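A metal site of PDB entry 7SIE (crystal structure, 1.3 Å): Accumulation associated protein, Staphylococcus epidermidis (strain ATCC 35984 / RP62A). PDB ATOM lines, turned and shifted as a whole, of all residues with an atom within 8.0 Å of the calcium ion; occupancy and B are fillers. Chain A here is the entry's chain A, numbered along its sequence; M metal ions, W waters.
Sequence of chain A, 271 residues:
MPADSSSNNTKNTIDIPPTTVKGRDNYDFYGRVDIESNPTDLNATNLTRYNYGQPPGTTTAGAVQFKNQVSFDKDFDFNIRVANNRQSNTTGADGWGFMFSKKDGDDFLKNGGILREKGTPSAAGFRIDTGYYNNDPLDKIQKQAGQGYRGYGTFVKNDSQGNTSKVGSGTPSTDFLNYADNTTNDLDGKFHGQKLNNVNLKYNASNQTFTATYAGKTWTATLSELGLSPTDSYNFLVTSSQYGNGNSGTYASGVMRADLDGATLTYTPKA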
ATOM      1  N   ASN A  89      -0.569 -34.631 -18.574  1.00  0.00           N
ATOM      2  CA  ASN A  89       0.142 -34.100 -19.732  1.00  0.00           C
ATOM      3  C   ASN A  89       1.310 -34.968 -20.153  1.00  0.00           C
ATOM      4  O   ASN A  89       1.885 -34.715 -21.207  1.00  0.00           O
ATOM      5  CB  ASN A  89       0.536 -32.638 -19.547  1.00  0.00           C
ATOM      6  CG  ASN A  89       1.633 -32.380 -18.556  1.00  0.00           C
ATOM      7  OD1 ASN A  89       2.360 -33.296 -18.173  1.00  0.00           O
ATOM      8  ND2 ASN A  89       1.783 -31.129 -18.206  1.00  0.00           N
ATOM      9  N   ALA A  93      -2.832 -36.341 -25.111  1.00  0.00           N
ATOM     10  CA  ALA A  93      -2.499 -35.768 -26.408  1.00  0.00           C
ATOM     11  C   ALA A  93      -1.636 -34.510 -26.282  1.00  0.00           C
ATOM     12  O   ALA A  93      -1.498 -33.938 -25.205  1.00  0.00           O
ATOM     13  CB  ALA A  93      -3.789 -35.445 -27.141  1.00  0.00           C
ATOM     14  N   ASP A  94      -1.112 -34.094 -27.415  1.00  0.00           N
ATOM     15  CA  ASP A  94      -0.244 -32.904 -27.468  1.00  0.00           C
ATOM     16  C   ASP A  94      -1.029 -31.614 -27.308  1.00  0.00           C
ATOM     17  O   ASP A  94      -0.487 -30.625 -26.808  1.00  0.00           O
ATOM     18  CB  ASP A  94       0.513 -32.930 -28.788  1.00  0.00           C
ATOM     19  CG  ASP A  94       1.390 -34.154 -28.955  1.00  0.00           C
ATOM     20  OD1 ASP A  94       1.887 -34.659 -27.916  1.00  0.00           O
ATOM     21  OD2 ASP A  94       1.594 -34.614 -30.070  1.00  0.00           O
ATOM     22  N   GLY A  95      -2.269 -31.588 -27.797  1.00  0.00           N
ATOM     23  CA  GLY A  95      -3.116 -30.419 -27.743  1.00  0.00           C
ATOM     24  C   GLY A  95      -3.870 -30.227 -29.036  1.00  0.00           C
ATOM     25  O   GLY A  95      -4.133 -31.180 -29.757  1.00  0.00           O
ATOM     26  N   ILE A 114       1.938 -27.166 -35.211  1.00  0.00           N
ATOM     27  CA  ILE A 114       2.256 -26.045 -34.311  1.00  0.00           C
ATOM     28  C   ILE A 114       2.160 -26.439 -32.850  1.00  0.00           C
ATOM     29  O   ILE A 114       2.039 -25.543 -31.990  1.00  0.00           O
ATOM     30  CB  ILE A 114       1.421 -24.819 -34.675  1.00  0.00           C
ATOM     31  CG1 ILE A 114      -0.084 -25.081 -34.604  1.00  0.00           C
ATOM     32  CG2 ILE A 114       1.864 -24.211 -35.997  1.00  0.00           C
ATOM     33  CD1 ILE A 114      -0.937 -23.828 -34.605  1.00  0.00           C
ATOM     34  N   LEU A 115       2.274 -27.737 -32.520  1.00  0.00           N
ATOM     35  CA  LEU A 115       2.169 -28.244 -31.172  1.00  0.00           C
ATOM     36  C   LEU A 115       3.497 -28.662 -30.552  1.00  0.00           C
ATOM     37  O   LEU A 115       3.492 -29.173 -29.427  1.00  0.00           O
ATOM     38  CB  LEU A 115       1.137 -29.386 -31.115  1.00  0.00           C
ATOM     39  CG  LEU A 115      -0.307 -28.916 -31.044  1.00  0.00           C
ATOM     40  CD1 LEU A 115      -1.257 -30.010 -31.410  1.00  0.00           C
ATOM     41  CD2 LEU A 115      -0.604 -28.394 -29.639  1.00  0.00           C
ATOM     42  N   ARG A 116       4.593 -28.533 -31.294  1.00  0.00           N
ATOM     43  CA  ARG A 116       5.938 -29.002 -30.867  1.00  0.00           C
ATOM     44  C   ARG A 116       6.924 -27.858 -31.085  1.00  0.00           C
ATOM     45  O   ARG A 116       6.564 -26.685 -31.084  1.00  0.00           O
ATOM     46  CB  ARG A 116       6.239 -30.292 -31.609  1.00  0.00           C
ATOM     47  CG  ARG A 116       5.470 -31.492 -31.063  1.00  0.00           C
ATOM     48  CD  ARG A 116       6.035 -31.851 -29.672  1.00  0.00           C
ATOM     49  NE  ARG A 116       5.486 -33.031 -29.032  1.00  0.00           N
ATOM     50  CZ  ARG A 116       5.980 -34.272 -29.129  1.00  0.00           C
ATOM     51  NH1 ARG A 116       6.963 -34.633 -29.962  1.00  0.00           N
ATOM     52  NH2 ARG A 116       5.398 -35.170 -28.407  1.00  0.00           N
ATOM     53  N   GLU A 117       8.194 -28.227 -31.237  1.00  0.00           N
ATOM     54  CA  GLU A 117       9.312 -27.296 -31.428  1.00  0.00           C
ATOM     55  C   GLU A 117       9.551 -27.028 -32.892  1.00  0.00           C
ATOM     56  O   GLU A 117      10.263 -26.046 -33.218  1.00  0.00           O
ATOM     57  CB  GLU A 117      10.574 -27.804 -30.735  1.00  0.00           C
ATOM     58  CG  GLU A 117      11.425 -28.846 -31.444  1.00  0.00           C
ATOM     59  CD  GLU A 117      10.888 -30.232 -31.667  1.00  0.00           C
ATOM     60  OE1 GLU A 117       9.726 -30.532 -31.234  1.00  0.00           O
ATOM     61  OE2 GLU A 117      11.693 -31.042 -32.160  1.00  0.00           O
ATOM     62  N   ARG A 127      -2.325 -22.284 -30.557  1.00  0.00           N
ATOM     63  CA  ARG A 127      -1.934 -23.538 -29.899  1.00  0.00           C
ATOM     64  C   ARG A 127      -2.594 -23.642 -28.526  1.00  0.00           C
ATOM     65  O   ARG A 127      -2.382 -22.753 -27.681  1.00  0.00           O
ATOM     66  CB  ARG A 127      -0.404 -23.488 -29.770  1.00  0.00           C
ATOM     67  CG  ARG A 127       0.252 -24.700 -29.108  1.00  0.00           C
ATOM     68  CD  ARG A 127       1.711 -24.340 -28.856  1.00  0.00           C
ATOM     69  NE  ARG A 127       2.541 -25.402 -28.291  1.00  0.00           N
ATOM     70  CZ  ARG A 127       3.765 -25.721 -28.750  1.00  0.00           C
ATOM     71  NH1 ARG A 127       4.104 -25.473 -30.016  1.00  0.00           N
ATOM     72  NH2 ARG A 127       4.609 -26.322 -27.939  1.00  0.00           N
ATOM     73  N   ILE A 128      -3.355 -24.692 -28.322  1.00  0.00           N
ATOM     74  CA  ILE A 128      -3.849 -25.080 -26.987  1.00  0.00           C
ATOM     75  C   ILE A 128      -3.027 -26.307 -26.635  1.00  0.00           C
ATOM     76  O   ILE A 128      -3.246 -27.393 -27.179  1.00  0.00           O
ATOM     77  CB  ILE A 128      -5.348 -25.363 -26.905  1.00  0.00           C
ATOM     78  CG1 ILE A 128      -6.164 -24.156 -27.373  1.00  0.00           C
ATOM     79  CG2 ILE A 128      -5.700 -25.783 -25.484  1.00  0.00           C
ATOM     80  CD1 ILE A 128      -7.649 -24.408 -27.458  1.00  0.00           C
ATOM     81  N   ASP A 129      -2.023 -26.123 -25.769  1.00  0.00           N
ATOM     82  CA  ASP A 129      -1.011 -27.122 -25.491  1.00  0.00           C
ATOM     83  C   ASP A 129      -1.418 -27.922 -24.259  1.00  0.00           C
ATOM     84  O   ASP A 129      -1.553 -27.350 -23.171  1.00  0.00           O
ATOM     85  CB  ASP A 129       0.324 -26.443 -25.331  1.00  0.00           C
ATOM     86  CG  ASP A 129       1.455 -27.427 -25.322  1.00  0.00           C
ATOM     87  OD1 ASP A 129       1.324 -28.482 -24.665  1.00  0.00           O
ATOM     88  OD2 ASP A 129       2.502 -27.159 -25.959  1.00  0.00           O
ATOM     89  N   THR A 130      -1.617 -29.228 -24.421  1.00  0.00           N
ATOM     90  CA  THR A 130      -2.039 -30.133 -23.353  1.00  0.00           C
ATOM     91  C   THR A 130      -1.058 -31.255 -23.055  1.00  0.00           C
ATOM     92  O   THR A 130      -1.328 -32.053 -22.144  1.00  0.00           O
ATOM     93  CB  THR A 130      -3.431 -30.720 -23.634  1.00  0.00           C
ATOM     94  OG1 THR A 130      -3.352 -31.547 -24.813  1.00  0.00           O
ATOM     95  CG2 THR A 130      -4.456 -29.652 -23.918  1.00  0.00           C
ATOM     96  N   GLY A 131       0.059 -31.315 -23.780  1.00  0.00           N
ATOM     97  CA  GLY A 131       0.987 -32.424 -23.636  1.00  0.00           C
ATOM     98  C   GLY A 131       2.408 -31.971 -23.457  1.00  0.00           C
ATOM     99  O   GLY A 131       2.892 -31.120 -24.243  1.00  0.00           O
ATOM    100  N   TYR A 132       3.112 -32.507 -22.458  1.00  0.00           N
ATOM    101  CA  TYR A 132       4.504 -32.157 -22.211  1.00  0.00           C
ATOM    102  C   TYR A 132       5.413 -32.944 -23.143  1.00  0.00           C
ATOM    103  O   TYR A 132       5.299 -34.170 -23.246  1.00  0.00           O
ATOM    104  CB  TYR A 132       4.809 -32.477 -20.740  1.00  0.00           C
ATOM    105  CG  TYR A 132       6.252 -32.241 -20.434  1.00  0.00           C
ATOM    106  CD1 TYR A 132       6.697 -30.955 -20.212  1.00  0.00           C
ATOM    107  CD2 TYR A 132       7.177 -33.255 -20.408  1.00  0.00           C
ATOM    108  CE1 TYR A 132       8.052 -30.680 -19.998  1.00  0.00           C
ATOM    109  CE2 TYR A 132       8.529 -32.999 -20.182  1.00  0.00           C
ATOM    110  CZ  TYR A 132       8.977 -31.699 -19.964  1.00  0.00           C
ATOM    111  OH  TYR A 132      10.291 -31.401 -19.784  1.00  0.00           O
ATOM    112  N   TYR A 133       6.382 -32.256 -23.697  1.00  0.00           N
ATOM    113  CA  TYR A 133       7.467 -32.872 -24.492  1.00  0.00           C
ATOM    114  C   TYR A 133       8.810 -32.423 -23.945  1.00  0.00           C
ATOM    115  O   TYR A 133       9.085 -31.223 -23.902  1.00  0.00           O
ATOM    116  CB  TYR A 133       7.288 -32.547 -25.971  1.00  0.00           C
ATOM    117  CG  TYR A 133       8.345 -33.180 -26.846  1.00  0.00           C
ATOM    118  CD1 TYR A 133       8.670 -34.492 -26.754  1.00  0.00           C
ATOM    119  CD2 TYR A 133       9.020 -32.447 -27.804  1.00  0.00           C
ATOM    120  CE1 TYR A 133       9.637 -35.074 -27.554  1.00  0.00           C
ATOM    121  CE2 TYR A 133       9.962 -32.993 -28.629  1.00  0.00           C
ATOM    122  CZ  TYR A 133      10.286 -34.320 -28.511  1.00  0.00           C
ATOM    123  OH  TYR A 133      11.276 -34.867 -29.301  1.00  0.00           O
ATOM    124  N   ASN A 134       9.673 -33.381 -23.621  1.00  0.00           N
ATOM    125  CA  ASN A 134      10.949 -33.085 -22.955  1.00  0.00           C
ATOM    126  C   ASN A 134      11.895 -32.273 -23.808  1.00  0.00           C
ATOM    127  O   ASN A 134      12.820 -31.717 -23.235  1.00  0.00           O
ATOM    128  CB  ASN A 134      11.565 -34.368 -22.416  1.00  0.00           C
ATOM    129  CG  ASN A 134      12.382 -34.158 -21.120  1.00  0.00           C
ATOM    130  OD1 ASN A 134      11.970 -33.437 -20.190  1.00  0.00           O
ATOM    131  ND2 ASN A 134      13.508 -34.745 -20.994  1.00  0.00           N
ATOM    132  N   ASP A 136      10.897 -29.778 -25.979  1.00  0.00           N
ATOM    133  CA  ASP A 136      10.262 -28.553 -26.471  1.00  0.00           C
ATOM    134  C   ASP A 136      10.634 -27.382 -25.587  1.00  0.00           C
ATOM    135  O   ASP A 136      10.181 -27.303 -24.431  1.00  0.00           O
ATOM    136  CB  ASP A 136       8.761 -28.753 -26.549  1.00  0.00           C
ATOM    137  CG  ASP A 136       8.045 -27.621 -27.245  1.00  0.00           C
ATOM    138  OD1 ASP A 136       8.548 -26.496 -27.222  1.00  0.00           O
ATOM    139  OD2 ASP A 136       7.015 -27.883 -27.879  1.00  0.00           O
ATOM    140  N   LEU A 138       9.565 -24.381 -25.517  1.00  0.00           N
ATOM    141  CA  LEU A 138       8.400 -23.569 -25.106  1.00  0.00           C
ATOM    142  C   LEU A 138       7.711 -24.252 -23.933  1.00  0.00           C
ATOM    143  O   LEU A 138       7.243 -23.564 -23.034  1.00  0.00           O
ATOM    144  CB  LEU A 138       7.448 -23.368 -26.267  1.00  0.00           C
ATOM    145  CG  LEU A 138       6.303 -22.381 -26.043  1.00  0.00           C
ATOM    146  CD1 LEU A 138       6.772 -21.005 -25.572  1.00  0.00           C
ATOM    147  CD2 LEU A 138       5.448 -22.311 -27.292  1.00  0.00           C
ATOM    148  N   ASP A 139       7.669 -25.582 -23.865  1.00  0.00           N
ATOM    149  CA  ASP A 139       7.085 -26.251 -22.719  1.00  0.00           C
ATOM    150  C   ASP A 139       7.864 -25.904 -21.446  1.00  0.00           C
ATOM    151  O   ASP A 139       7.253 -25.844 -20.382  1.00  0.00           O
ATOM    152  CB  ASP A 139       7.064 -27.761 -22.918  1.00  0.00           C
ATOM    153  CG  ASP A 139       6.034 -28.258 -23.921  1.00  0.00           C
ATOM    154  OD1 ASP A 139       5.328 -27.420 -24.558  1.00  0.00           O
ATOM    155  OD2 ASP A 139       5.879 -29.483 -24.082  1.00  0.00           O
ATOM    156  N   LYS A 140       9.164 -25.715 -21.549  1.00  0.00           N
ATOM    157  CA  LYS A 140       9.975 -25.291 -20.405  1.00  0.00           C
ATOM    158  C   LYS A 140       9.641 -23.875 -19.961  1.00  0.00           C
ATOM    159  O   LYS A 140       9.506 -23.650 -18.718  1.00  0.00           O
ATOM    160  CB  LYS A 140      11.461 -25.426 -20.743  1.00  0.00           C
ATOM    161  CG  LYS A 140      11.972 -26.834 -20.568  1.00  0.00           C
ATOM    162  CD  LYS A 140      13.469 -26.931 -20.768  1.00  0.00           C
ATOM    163  CE  LYS A 140      13.919 -28.362 -20.931  1.00  0.00           C
ATOM    164  NZ  LYS A 140      13.126 -29.133 -21.930  1.00  0.00           N
ATOM    165  N   GLN A 142       6.959 -22.281 -20.420  1.00  0.00           N
ATOM    166  CA  GLN A 142       5.561 -22.206 -19.954  1.00  0.00           C
ATOM    167  C   GLN A 142       5.321 -23.001 -18.671  1.00  0.00           C
ATOM    168  O   GLN A 142       4.199 -23.083 -18.180  1.00  0.00           O
ATOM    169  CB  GLN A 142       4.601 -22.668 -21.040  1.00  0.00           C
ATOM    170  CG  GLN A 142       4.661 -21.903 -22.342  1.00  0.00           C
ATOM    171  CD  GLN A 142       4.177 -20.483 -22.243  1.00  0.00           C
ATOM    172  OE1 GLN A 142       4.705 -19.683 -21.495  1.00  0.00           O
ATOM    173  NE2 GLN A 142       3.207 -20.160 -23.079  1.00  0.00           N
ATOM    174  N   GLN A 144       5.245 -26.179 -18.156  1.00  0.00           N
ATOM    175  CA  GLN A 144       4.253 -27.250 -18.370  1.00  0.00           C
ATOM    176  C   GLN A 144       4.487 -28.474 -17.497  1.00  0.00           C
ATOM    177  O   GLN A 144       3.512 -29.115 -17.124  1.00  0.00           O
ATOM    178  CB  GLN A 144       4.136 -27.553 -19.857  1.00  0.00           C
ATOM    179  CG  GLN A 144       3.102 -28.609 -20.155  1.00  0.00           C
ATOM    180  CD  GLN A 144       2.707 -28.697 -21.598  1.00  0.00           C
ATOM    181  OE1 GLN A 144       3.553 -28.599 -22.522  1.00  0.00           O
ATOM    182  NE2 GLN A 144       1.415 -28.887 -21.831  1.00  0.00           N
ATOM    183  N   ARG A 150      -1.695 -29.649 -16.686  1.00  0.00           N
ATOM    184  CA  ARG A 150      -0.975 -28.416 -16.945  1.00  0.00           C
ATOM    185  C   ARG A 150      -0.789 -28.206 -18.443  1.00  0.00           C
ATOM    186  O   ARG A 150      -0.160 -29.002 -19.138  1.00  0.00           O
ATOM    187  CB  ARG A 150       0.391 -28.399 -16.280  1.00  0.00           C
ATOM    188  CG  ARG A 150       0.359 -28.488 -14.756  1.00  0.00           C
ATOM    189  CD  ARG A 150       1.750 -28.456 -14.152  1.00  0.00           C
ATOM    190  NE  ARG A 150       2.473 -27.213 -14.348  1.00  0.00           N
ATOM    191  CZ  ARG A 150       2.321 -26.149 -13.588  1.00  0.00           C
ATOM    192  NH1 ARG A 150       1.455 -26.132 -12.597  1.00  0.00           N
ATOM    193  NH2 ARG A 150       3.060 -25.101 -13.794  1.00  0.00           N
ATOM    194  N   GLY A 151      -1.257 -27.046 -18.891  1.00  0.00           N
ATOM    195  CA  GLY A 151      -1.050 -26.669 -20.291  1.00  0.00           C
ATOM    196  C   GLY A 151      -1.033 -25.165 -20.431  1.00  0.00           C
ATOM    197  O   GLY A 151      -0.800 -24.420 -19.461  1.00  0.00           O
ATOM    198  N   TYR A 152      -1.210 -24.727 -21.647  1.00  0.00           N
ATOM    199  CA  TYR A 152      -1.119 -23.274 -21.955  1.00  0.00           C
ATOM    200  C   TYR A 152      -1.760 -23.030 -23.287  1.00  0.00           C
ATOM    201  O   TYR A 152      -1.835 -23.921 -24.133  1.00  0.00           O
ATOM    202  CB  TYR A 152       0.328 -22.757 -21.924  1.00  0.00           C
ATOM    203  CG  TYR A 152       1.318 -23.453 -22.836  1.00  0.00           C
ATOM    204  CD1 TYR A 152       2.045 -24.544 -22.405  1.00  0.00           C
ATOM    205  CD2 TYR A 152       1.565 -22.995 -24.131  1.00  0.00           C
ATOM    206  CE1 TYR A 152       3.047 -25.123 -23.190  1.00  0.00           C
ATOM    207  CE2 TYR A 152       2.558 -23.544 -24.899  1.00  0.00           C
ATOM    208  CZ  TYR A 152       3.329 -24.584 -24.415  1.00  0.00           C
ATOM    209  OH  TYR A 152       4.375 -25.018 -25.185  1.00  0.00           O
HETATM  210 CA    CA M   1       3.642 -29.129 -25.067  1.00  0.00          CA
HETATM  211  O   HOH W   1       2.296 -30.114 -27.028  1.00  0.00           O
HETATM  212  O   HOH W   2       4.986 -29.459 -27.038  1.00  0.00           O
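OD1 of Asp 139 sits close to OH of Tyr 152 (2.7 Å). The backbone NH (N) of Gly 131 lies close to the backbone carbonyl oxygen (O) of Ala 93, 3.4 Å away. O of Asp 94 lies within hydrogen-bond range of N of Gly 131, 3.2 Å away. NE2 of Gln 144 lies within hydrogen-bond range of O of Arg 150, at 3.1 Å. ND2 of Asn 89 lies within hydrogen-bond range of O of Gln 144 (2.9 Å). OD2 of Asp 139 lies close to N of Tyr 133, at 2.8 Å. OD2 of Asp 129 sits close to NE of Arg 127 (2.9 Å). NH2 of Arg 127 lies close to OD1 of Asp 139.
Within 4 Å of the calcium ion: Asp 129, Gly 131, Asp 139 and Gln 144. The nearest printed residue that does not touch the calcium ion is Arg 127 (4.1 Å).
The calcium ion is bound by the backbone carbonyl oxygen (O) of Gly 131 (2.3 Å), water W2 (2.4 Å), the side-chain carboxylate (OD1) of Asp 129 (2.4 Å), the side-chain carboxylate (OD2) of Asp 129 (2.4 Å), the side-chain carboxylate (OD1) of Asp 139 (2.5 Å), the side-chain carboxylate (OD2) of Asp 139 (2.5 Å), water W1 (2.6 Å) and the side-chain amide oxygen (OE1) of Gln 144 (2.6 Å).
Water W1 lies within hydrogen-bond range of O of Asp 94 and O of Leu 115. Water W2 lies within hydrogen-bond range of the side-chain carboxylate of Asp 136 (2.7 Å), the backbone carbonyl oxygen of Leu 115 (2.8 Å) and the guanidinium group of Arg 127 (3.3 Å).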
